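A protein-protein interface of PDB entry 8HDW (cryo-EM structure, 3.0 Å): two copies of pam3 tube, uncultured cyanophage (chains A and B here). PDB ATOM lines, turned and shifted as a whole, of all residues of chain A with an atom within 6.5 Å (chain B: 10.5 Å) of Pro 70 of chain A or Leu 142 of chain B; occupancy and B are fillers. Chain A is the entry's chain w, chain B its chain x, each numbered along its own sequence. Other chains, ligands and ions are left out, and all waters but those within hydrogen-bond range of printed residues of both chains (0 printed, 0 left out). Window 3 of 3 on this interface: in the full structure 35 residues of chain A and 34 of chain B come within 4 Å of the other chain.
Among the printed residues, merely in contact across the chains: Pro 67 of chain A with Glu 101 of chain B (3.6 Å), Pro 67 of chain A with Leu 142 of chain B (3.9 Å), Asn 68 of chain A with Leu 142 of chain B (3.8 Å), Ser 69 of chain A with Leu 142 of chain B (3.8 Å), Pro 70 of chain A with Leu 142 of chain B (3.8 Å), Arg 73 of chain A with Ile 138 of chain B (3.98 Å), Arg 73 of chain A with Thr 140 of chain B (3.4 Å) and Arg 73 of chain A with Leu 142 of chain B (3.8 Å).
Hydrophobic or aromatic side chains of chain B that line the printed part of chain A: Ile 138 and Leu 142. Among the printed residues, no Asp or Glu carboxylate lies within 4 Å of a Lys or Arg side-chain nitrogen of the other chain.
O of Pro 139 of chain B lies close to NE of Arg 73 of chain A, at 3.5 Å. OE2 of Glu 101 of chain B sits at hydrogen-bond distance from NE2 of His 72 of chain A, 3.5 Å away.
No position is printed for both chains. Of the 10 pairs that touch across the chains among the printed residues, none has its exchanged pair printed and touching as well.
Pro 70 of chain A touches one residue of chain B. No residue of chain B comes within 4 Å of Thr 71 of chain A. Of the printed residues of chain B, His 72 of chain A touches Glu 101 (3.5 Å). Of the printed residues of chain A, Glu 101 of chain B touches Pro 67 and His 72. Of the printed residues of chain A, Pro 139 of chain B touches Arg 73 (3.3 Å). Printed residues of chain A within 4 Å of Thr 140 of chain B: Arg 73 (3.4 Å). Leu 142 of chain B touches just these residues of chain A: Pro 67 (3.9 Å), Asn 68 (3.8 Å), Ser 69 (3.8 Å), Pro 70 (3.8 Å) and Arg 73 (3.8 Å). The nearest residue of chain B that does not touch Pro 70 of chain A is Pro 139 of chain B (7.0 Å). The nearest printed residue of chain A that does not touch Thr 140 of chain B is Pro 70 of chain A (8.7 Å).
The side-chain amide nitrogen (ND2) of Asn 100 of chain B sits at hydrogen-bond distance from the side-chain hydroxyl (OG1) of Thr 140 of chain B (3.3 Å). The backbone NH of Asp 96 of chain B sits at hydrogen-bond distance from the backbone carbonyl oxygen of Glu 101 of chain B (3.0 Å).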
ATOM      1  N   ARG A  18      -2.780  11.609  20.825  1.00  0.00           N
ATOM      2  CA  ARG A  18      -1.605  11.292  21.621  1.00  0.00           C
ATOM      3  C   ARG A  18      -0.351  11.896  20.996  1.00  0.00           C
ATOM      4  O   ARG A  18      -0.305  12.195  19.804  1.00  0.00           O
ATOM      5  CB  ARG A  18      -1.446   9.780  21.761  1.00  0.00           C
ATOM      6  CG  ARG A  18      -2.703   9.078  22.210  1.00  0.00           C
ATOM      7  CD  ARG A  18      -2.395   7.971  23.200  1.00  0.00           C
ATOM      8  NE  ARG A  18      -2.143   6.698  22.537  1.00  0.00           N
ATOM      9  CZ  ARG A  18      -3.072   5.772  22.330  1.00  0.00           C
ATOM     10  NH1 ARG A  18      -4.314   5.978  22.742  1.00  0.00           N
ATOM     11  NH2 ARG A  18      -2.764   4.641  21.715  1.00  0.00           N
ATOM     12  N   ILE A  21       6.488  10.178  20.159  1.00  0.00           N
ATOM     13  CA  ILE A  21       7.582  10.197  21.125  1.00  0.00           C
ATOM     14  C   ILE A  21       8.900   9.640  20.589  1.00  0.00           C
ATOM     15  O   ILE A  21       9.867  10.389  20.427  1.00  0.00           O
ATOM     16  CB  ILE A  21       7.163   9.468  22.412  1.00  0.00           C
ATOM     17  CG1 ILE A  21       5.948   8.589  22.147  1.00  0.00           C
ATOM     18  CG2 ILE A  21       6.847  10.472  23.503  1.00  0.00           C
ATOM     19  CD1 ILE A  21       5.288   8.069  23.398  1.00  0.00           C
ATOM     20  N   GLY A  22       8.970   8.351  20.291  1.00  0.00           N
ATOM     21  CA  GLY A  22      10.284   7.812  19.987  1.00  0.00           C
ATOM     22  C   GLY A  22      10.685   7.930  18.533  1.00  0.00           C
ATOM     23  O   GLY A  22      10.371   7.060  17.723  1.00  0.00           O
ATOM     24  N   LEU A  65      10.616   6.146  13.156  1.00  0.00           N
ATOM     25  CA  LEU A  65      10.537   5.781  14.559  1.00  0.00           C
ATOM     26  C   LEU A  65      11.584   4.731  14.893  1.00  0.00           C
ATOM     27  O   LEU A  65      12.134   4.072  14.008  1.00  0.00           O
ATOM     28  CB  LEU A  65       9.148   5.237  14.915  1.00  0.00           C
ATOM     29  CG  LEU A  65       7.937   6.140  14.697  1.00  0.00           C
ATOM     30  CD1 LEU A  65       6.674   5.354  14.902  1.00  0.00           C
ATOM     31  CD2 LEU A  65       7.972   7.336  15.623  1.00  0.00           C
ATOM     32  N   PRO A  67      12.496   1.073  16.867  1.00  0.00           N
ATOM     33  CA  PRO A  67      11.747  -0.165  17.123  1.00  0.00           C
ATOM     34  C   PRO A  67      11.146  -0.262  18.518  1.00  0.00           C
ATOM     35  O   PRO A  67      10.339  -1.167  18.747  1.00  0.00           O
ATOM     36  CB  PRO A  67      12.789  -1.266  16.882  1.00  0.00           C
ATOM     37  CG  PRO A  67      14.100  -0.581  16.840  1.00  0.00           C
ATOM     38  CD  PRO A  67      13.854   0.800  16.378  1.00  0.00           C
ATOM     39  N   ASN A  68      11.507   0.616  19.454  1.00  0.00           N
ATOM     40  CA  ASN A  68      10.914   0.626  20.792  1.00  0.00           C
ATOM     41  C   ASN A  68      10.251   1.977  21.051  1.00  0.00           C
ATOM     42  O   ASN A  68      10.795   2.830  21.751  1.00  0.00           O
ATOM     43  CB  ASN A  68      11.982   0.313  21.852  1.00  0.00           C
ATOM     44  CG  ASN A  68      13.074   1.363  21.918  1.00  0.00           C
ATOM     45  OD1 ASN A  68      13.427   1.966  20.914  1.00  0.00           O
ATOM     46  ND2 ASN A  68      13.592   1.600  23.109  1.00  0.00           N
ATOM     47  N   SER A  69       9.044   2.164  20.527  1.00  0.00           N
ATOM     48  CA  SER A  69       8.363   3.413  20.789  1.00  0.00           C
ATOM     49  C   SER A  69       6.867   3.152  20.826  1.00  0.00           C
ATOM     50  O   SER A  69       6.372   2.353  20.020  1.00  0.00           O
ATOM     51  CB  SER A  69       8.680   4.486  19.751  1.00  0.00           C
ATOM     52  OG  SER A  69       8.344   4.066  18.450  1.00  0.00           O
ATOM     53  N   PRO A  70       6.138   3.771  21.753  1.00  0.00           N
ATOM     54  CA  PRO A  70       4.689   3.535  21.826  1.00  0.00           C
ATOM     55  C   PRO A  70       3.934   3.951  20.579  1.00  0.00           C
ATOM     56  O   PRO A  70       2.866   3.395  20.296  1.00  0.00           O
ATOM     57  CB  PRO A  70       4.274   4.365  23.043  1.00  0.00           C
ATOM     58  CG  PRO A  70       5.508   4.480  23.851  1.00  0.00           C
ATOM     59  CD  PRO A  70       6.620   4.585  22.876  1.00  0.00           C
ATOM     60  N   THR A  71       4.455   4.920  19.824  1.00  0.00           N
ATOM     61  CA  THR A  71       3.802   5.325  18.586  1.00  0.00           C
ATOM     62  C   THR A  71       3.838   4.215  17.547  1.00  0.00           C
ATOM     63  O   THR A  71       2.919   4.100  16.733  1.00  0.00           O
ATOM     64  CB  THR A  71       4.457   6.593  18.054  1.00  0.00           C
ATOM     65  OG1 THR A  71       4.542   7.548  19.113  1.00  0.00           O
ATOM     66  CG2 THR A  71       3.644   7.187  16.932  1.00  0.00           C
ATOM     67  N   HIS A  72       4.877   3.379  17.569  1.00  0.00           N
ATOM     68  CA  HIS A  72       4.910   2.211  16.696  1.00  0.00           C
ATOM     69  C   HIS A  72       3.772   1.249  17.024  1.00  0.00           C
ATOM     70  O   HIS A  72       3.119   0.716  16.120  1.00  0.00           O
ATOM     71  CB  HIS A  72       6.272   1.527  16.818  1.00  0.00           C
ATOM     72  CG  HIS A  72       6.496   0.420  15.836  1.00  0.00           C
ATOM     73  ND1 HIS A  72       6.394   0.596  14.474  1.00  0.00           N
ATOM     74  CD2 HIS A  72       6.836  -0.877  16.021  1.00  0.00           C
ATOM     75  CE1 HIS A  72       6.648  -0.546  13.864  1.00  0.00           C
ATOM     76  NE2 HIS A  72       6.920  -1.455  14.780  1.00  0.00           N
ATOM     77  N   ARG A  73       3.500   1.039  18.313  1.00  0.00           N
ATOM     78  CA  ARG A  73       2.379   0.198  18.720  1.00  0.00           C
ATOM     79  C   ARG A  73       1.043   0.813  18.311  1.00  0.00           C
ATOM     80  O   ARG A  73       0.142   0.110  17.832  1.00  0.00           O
ATOM     81  CB  ARG A  73       2.432  -0.031  20.230  1.00  0.00           C
ATOM     82  CG  ARG A  73       1.467  -1.082  20.760  1.00  0.00           C
ATOM     83  CD  ARG A  73       0.704  -0.563  21.963  1.00  0.00           C
ATOM     84  NE  ARG A  73       0.754  -1.466  23.107  1.00  0.00           N
ATOM     85  CZ  ARG A  73      -0.228  -2.293  23.451  1.00  0.00           C
ATOM     86  NH1 ARG A  73      -1.343  -2.337  22.740  1.00  0.00           N
ATOM     87  NH2 ARG A  73      -0.098  -3.076  24.507  1.00  0.00           N
ATOM     88  N   GLN A  74       0.896   2.127  18.484  1.00  0.00           N
ATOM     89  CA  GLN A  74      -0.344   2.787  18.089  1.00  0.00           C
ATOM     90  C   GLN A  74      -0.583   2.666  16.587  1.00  0.00           C
ATOM     91  O   GLN A  74      -1.704   2.379  16.140  1.00  0.00           O
ATOM     92  CB  GLN A  74      -0.305   4.252  18.514  1.00  0.00           C
ATOM     93  CG  GLN A  74      -1.564   5.010  18.200  1.00  0.00           C
ATOM     94  CD  GLN A  74      -1.449   6.485  18.481  1.00  0.00           C
ATOM     95  OE1 GLN A  74      -0.364   6.997  18.728  1.00  0.00           O
ATOM     96  NE2 GLN A  74      -2.572   7.179  18.442  1.00  0.00           N
ATOM     97  N   LEU A  75       0.464   2.865  15.789  1.00  0.00           N
ATOM     98  CA  LEU A  75       0.312   2.800  14.341  1.00  0.00           C
ATOM     99  C   LEU A  75       0.070   1.375  13.865  1.00  0.00           C
ATOM    100  O   LEU A  75      -0.681   1.158  12.909  1.00  0.00           O
ATOM    101  CB  LEU A  75       1.535   3.403  13.663  1.00  0.00           C
ATOM    102  CG  LEU A  75       1.547   4.927  13.632  1.00  0.00           C
ATOM    103  CD1 LEU A  75       2.880   5.452  13.158  1.00  0.00           C
ATOM    104  CD2 LEU A  75       0.439   5.437  12.742  1.00  0.00           C
ATOM    105  N   MET B   1       9.218  -6.197  34.938  1.00  0.00           N
ATOM    106  CA  MET B   1       9.372  -6.534  33.528  1.00  0.00           C
ATOM    107  C   MET B   1      10.119  -5.429  32.789  1.00  0.00           C
ATOM    108  O   MET B   1       9.550  -4.729  31.949  1.00  0.00           O
ATOM    109  CB  MET B   1       8.008  -6.781  32.886  1.00  0.00           C
ATOM    110  CG  MET B   1       7.383  -8.114  33.263  1.00  0.00           C
ATOM    111  SD  MET B   1       5.642  -8.227  32.809  1.00  0.00           S
ATOM    112  CE  MET B   1       5.665  -7.575  31.142  1.00  0.00           C
ATOM    113  N   ALA B   2      11.402  -5.287  33.112  1.00  0.00           N
ATOM    114  CA  ALA B   2      12.213  -4.220  32.547  1.00  0.00           C
ATOM    115  C   ALA B   2      12.331  -4.371  31.036  1.00  0.00           C
ATOM    116  O   ALA B   2      12.449  -5.478  30.504  1.00  0.00           O
ATOM    117  CB  ALA B   2      13.605  -4.215  33.179  1.00  0.00           C
ATOM    118  N   MET B   3      12.290  -3.232  30.344  1.00  0.00           N
ATOM    119  CA  MET B   3      12.420  -3.213  28.894  1.00  0.00           C
ATOM    120  C   MET B   3      13.860  -3.548  28.527  1.00  0.00           C
ATOM    121  O   MET B   3      14.768  -2.742  28.753  1.00  0.00           O
ATOM    122  CB  MET B   3      11.996  -1.848  28.332  1.00  0.00           C
ATOM    123  CG  MET B   3      11.565  -1.833  26.868  1.00  0.00           C
ATOM    124  SD  MET B   3      12.912  -1.985  25.684  1.00  0.00           S
ATOM    125  CE  MET B   3      14.064  -0.767  26.314  1.00  0.00           C
ATOM    126  N   LYS B   4      14.085  -4.743  27.991  1.00  0.00           N
ATOM    127  CA  LYS B   4      15.432  -5.122  27.610  1.00  0.00           C
ATOM    128  C   LYS B   4      15.887  -4.329  26.390  1.00  0.00           C
ATOM    129  O   LYS B   4      15.161  -4.172  25.406  1.00  0.00           O
ATOM    130  CB  LYS B   4      15.517  -6.617  27.306  1.00  0.00           C
ATOM    131  CG  LYS B   4      15.832  -7.480  28.497  1.00  0.00           C
ATOM    132  CD  LYS B   4      15.928  -8.935  28.084  1.00  0.00           C
ATOM    133  CE  LYS B   4      14.674  -9.382  27.341  1.00  0.00           C
ATOM    134  NZ  LYS B   4      13.432  -9.192  28.143  1.00  0.00           N
ATOM    135  N   ALA B   5      17.122  -3.847  26.460  1.00  0.00           N
ATOM    136  CA  ALA B   5      17.767  -3.283  25.290  1.00  0.00           C
ATOM    137  C   ALA B   5      17.806  -4.325  24.181  1.00  0.00           C
ATOM    138  O   ALA B   5      17.610  -5.518  24.414  1.00  0.00           O
ATOM    139  CB  ALA B   5      19.173  -2.825  25.650  1.00  0.00           C
ATOM    140  N   ASP B  96      10.647 -10.891  18.748  1.00  0.00           N
ATOM    141  CA  ASP B  96      11.627 -10.344  19.674  1.00  0.00           C
ATOM    142  C   ASP B  96      11.037 -10.371  21.076  1.00  0.00           C
ATOM    143  O   ASP B  96       9.955  -9.829  21.304  1.00  0.00           O
ATOM    144  CB  ASP B  96      12.000  -8.916  19.278  1.00  0.00           C
ATOM    145  CG  ASP B  96      13.031  -8.305  20.191  1.00  0.00           C
ATOM    146  OD1 ASP B  96      13.700  -9.052  20.931  1.00  0.00           O
ATOM    147  OD2 ASP B  96      13.175  -7.068  20.173  1.00  0.00           O
ATOM    148  N   SER B  97      11.745 -11.000  22.014  1.00  0.00           N
ATOM    149  CA  SER B  97      11.217 -11.136  23.365  1.00  0.00           C
ATOM    150  C   SER B  97      11.261  -9.834  24.147  1.00  0.00           C
ATOM    151  O   SER B  97      10.551  -9.704  25.148  1.00  0.00           O
ATOM    152  CB  SER B  97      11.985 -12.210  24.129  1.00  0.00           C
ATOM    153  OG  SER B  97      11.759 -13.485  23.562  1.00  0.00           O
ATOM    154  N   ALA B  98      12.082  -8.874  23.727  1.00  0.00           N
ATOM    155  CA  ALA B  98      12.179  -7.618  24.453  1.00  0.00           C
ATOM    156  C   ALA B  98      10.952  -6.738  24.252  1.00  0.00           C
ATOM    157  O   ALA B  98      10.588  -5.982  25.156  1.00  0.00           O
ATOM    158  CB  ALA B  98      13.438  -6.865  24.029  1.00  0.00           C
ATOM    159  N   SER B  99      10.305  -6.820  23.090  1.00  0.00           N
ATOM    160  CA  SER B  99       9.189  -5.933  22.799  1.00  0.00           C
ATOM    161  C   SER B  99       7.953  -6.659  22.288  1.00  0.00           C
ATOM    162  O   SER B  99       6.901  -6.025  22.163  1.00  0.00           O
ATOM    163  CB  SER B  99       9.609  -4.873  21.785  1.00  0.00           C
ATOM    164  OG  SER B  99      10.155  -5.472  20.627  1.00  0.00           O
ATOM    165  N   ASN B 100       8.043  -7.960  22.004  1.00  0.00           N
ATOM    166  CA  ASN B 100       6.951  -8.743  21.417  1.00  0.00           C
ATOM    167  C   ASN B 100       6.585  -8.247  20.023  1.00  0.00           C
ATOM    168  O   ASN B 100       5.426  -8.296  19.618  1.00  0.00           O
ATOM    169  CB  ASN B 100       5.713  -8.764  22.314  1.00  0.00           C
ATOM    170  CG  ASN B 100       5.780  -9.835  23.378  1.00  0.00           C
ATOM    171  OD1 ASN B 100       6.372 -10.894  23.175  1.00  0.00           O
ATOM    172  ND2 ASN B 100       5.169  -9.567  24.524  1.00  0.00           N
ATOM    173  N   GLU B 101       7.576  -7.779  19.275  1.00  0.00           N
ATOM    174  CA  GLU B 101       7.374  -7.377  17.891  1.00  0.00           C
ATOM    175  C   GLU B 101       7.819  -8.495  16.955  1.00  0.00           C
ATOM    176  O   GLU B 101       8.853  -9.127  17.175  1.00  0.00           O
ATOM    177  CB  GLU B 101       8.139  -6.097  17.567  1.00  0.00           C
ATOM    178  CG  GLU B 101       7.908  -5.619  16.147  1.00  0.00           C
ATOM    179  CD  GLU B 101       8.882  -4.554  15.702  1.00  0.00           C
ATOM    180  OE1 GLU B 101       9.583  -3.983  16.559  1.00  0.00           O
ATOM    181  OE2 GLU B 101       8.945  -4.289  14.485  1.00  0.00           O
ATOM    182  N   GLY B 102       7.043  -8.728  15.915  1.00  0.00           N
ATOM    183  CA  GLY B 102       7.317  -9.798  14.983  1.00  0.00           C
ATOM    184  C   GLY B 102       6.096 -10.080  14.135  1.00  0.00           C
ATOM    185  O   GLY B 102       5.324  -9.182  13.829  1.00  0.00           O
ATOM    186  N   THR B 137       2.360  -9.189  14.858  1.00  0.00           N
ATOM    187  CA  THR B 137       1.981  -9.266  16.258  1.00  0.00           C
ATOM    188  C   THR B 137       2.110  -7.883  16.881  1.00  0.00           C
ATOM    189  O   THR B 137       2.944  -7.077  16.463  1.00  0.00           O
ATOM    190  CB  THR B 137       2.843 -10.289  17.005  1.00  0.00           C
ATOM    191  OG1 THR B 137       2.353 -10.455  18.338  1.00  0.00           O
ATOM    192  CG2 THR B 137       4.267  -9.840  17.074  1.00  0.00           C
ATOM    193  N   ILE B 138       1.258  -7.604  17.857  1.00  0.00           N
ATOM    194  CA  ILE B 138       1.245  -6.278  18.484  1.00  0.00           C
ATOM    195  C   ILE B 138       2.343  -6.210  19.539  1.00  0.00           C
ATOM    196  O   ILE B 138       2.392  -7.074  20.431  1.00  0.00           O
ATOM    197  CB  ILE B 138      -0.121  -5.997  19.099  1.00  0.00           C
ATOM    198  CG1 ILE B 138      -1.224  -6.160  18.054  1.00  0.00           C
ATOM    199  CG2 ILE B 138      -0.154  -4.605  19.688  1.00  0.00           C
ATOM    200  CD1 ILE B 138      -1.306  -5.031  17.068  1.00  0.00           C
ATOM    201  N   PRO B 139       3.241  -5.231  19.485  1.00  0.00           N
ATOM    202  CA  PRO B 139       4.236  -5.105  20.552  1.00  0.00           C
ATOM    203  C   PRO B 139       3.613  -4.578  21.830  1.00  0.00           C
ATOM    204  O   PRO B 139       3.438  -3.369  21.993  1.00  0.00           O
ATOM    205  CB  PRO B 139       5.247  -4.117  19.965  1.00  0.00           C
ATOM    206  CG  PRO B 139       4.474  -3.331  18.985  1.00  0.00           C
ATOM    207  CD  PRO B 139       3.465  -4.259  18.403  1.00  0.00           C
ATOM    208  N   THR B 140       3.315  -5.472  22.768  1.00  0.00           N
ATOM    209  CA  THR B 140       2.600  -5.062  23.968  1.00  0.00           C
ATOM    210  C   THR B 140       3.537  -4.506  25.026  1.00  0.00           C
ATOM    211  O   THR B 140       3.078  -3.889  25.992  1.00  0.00           O
ATOM    212  CB  THR B 140       1.799  -6.232  24.531  1.00  0.00           C
ATOM    213  OG1 THR B 140       2.640  -7.384  24.634  1.00  0.00           O
ATOM    214  CG2 THR B 140       0.628  -6.548  23.628  1.00  0.00           C
ATOM    215  N   LEU B 141       4.843  -4.707  24.860  1.00  0.00           N
ATOM    216  CA  LEU B 141       5.848  -4.125  25.737  1.00  0.00           C
ATOM    217  C   LEU B 141       6.438  -2.845  25.167  1.00  0.00           C
ATOM    218  O   LEU B 141       7.482  -2.382  25.643  1.00  0.00           O
ATOM    219  CB  LEU B 141       6.950  -5.145  26.016  1.00  0.00           C
ATOM    220  CG  LEU B 141       6.482  -6.567  26.320  1.00  0.00           C
ATOM    221  CD1 LEU B 141       7.666  -7.497  26.442  1.00  0.00           C
ATOM    222  CD2 LEU B 141       5.648  -6.605  27.577  1.00  0.00           C
ATOM    223  N   LEU B 142       5.799  -2.274  24.148  1.00  0.00           N
ATOM    224  CA  LEU B 142       6.253  -1.063  23.466  1.00  0.00           C
ATOM    225  C   LEU B 142       7.649  -1.243  22.876  1.00  0.00           C
ATOM    226  O   LEU B 142       7.811  -1.302  21.660  1.00  0.00           O
ATOM    227  CB  LEU B 142       6.229   0.133  24.420  1.00  0.00           C
ATOM    228  CG  LEU B 142       4.959   0.305  25.255  1.00  0.00           C
ATOM    229  CD1 LEU B 142       5.091   1.493  26.203  1.00  0.00           C
ATOM    230  CD2 LEU B 142       3.736   0.457  24.372  1.00  0.00           C
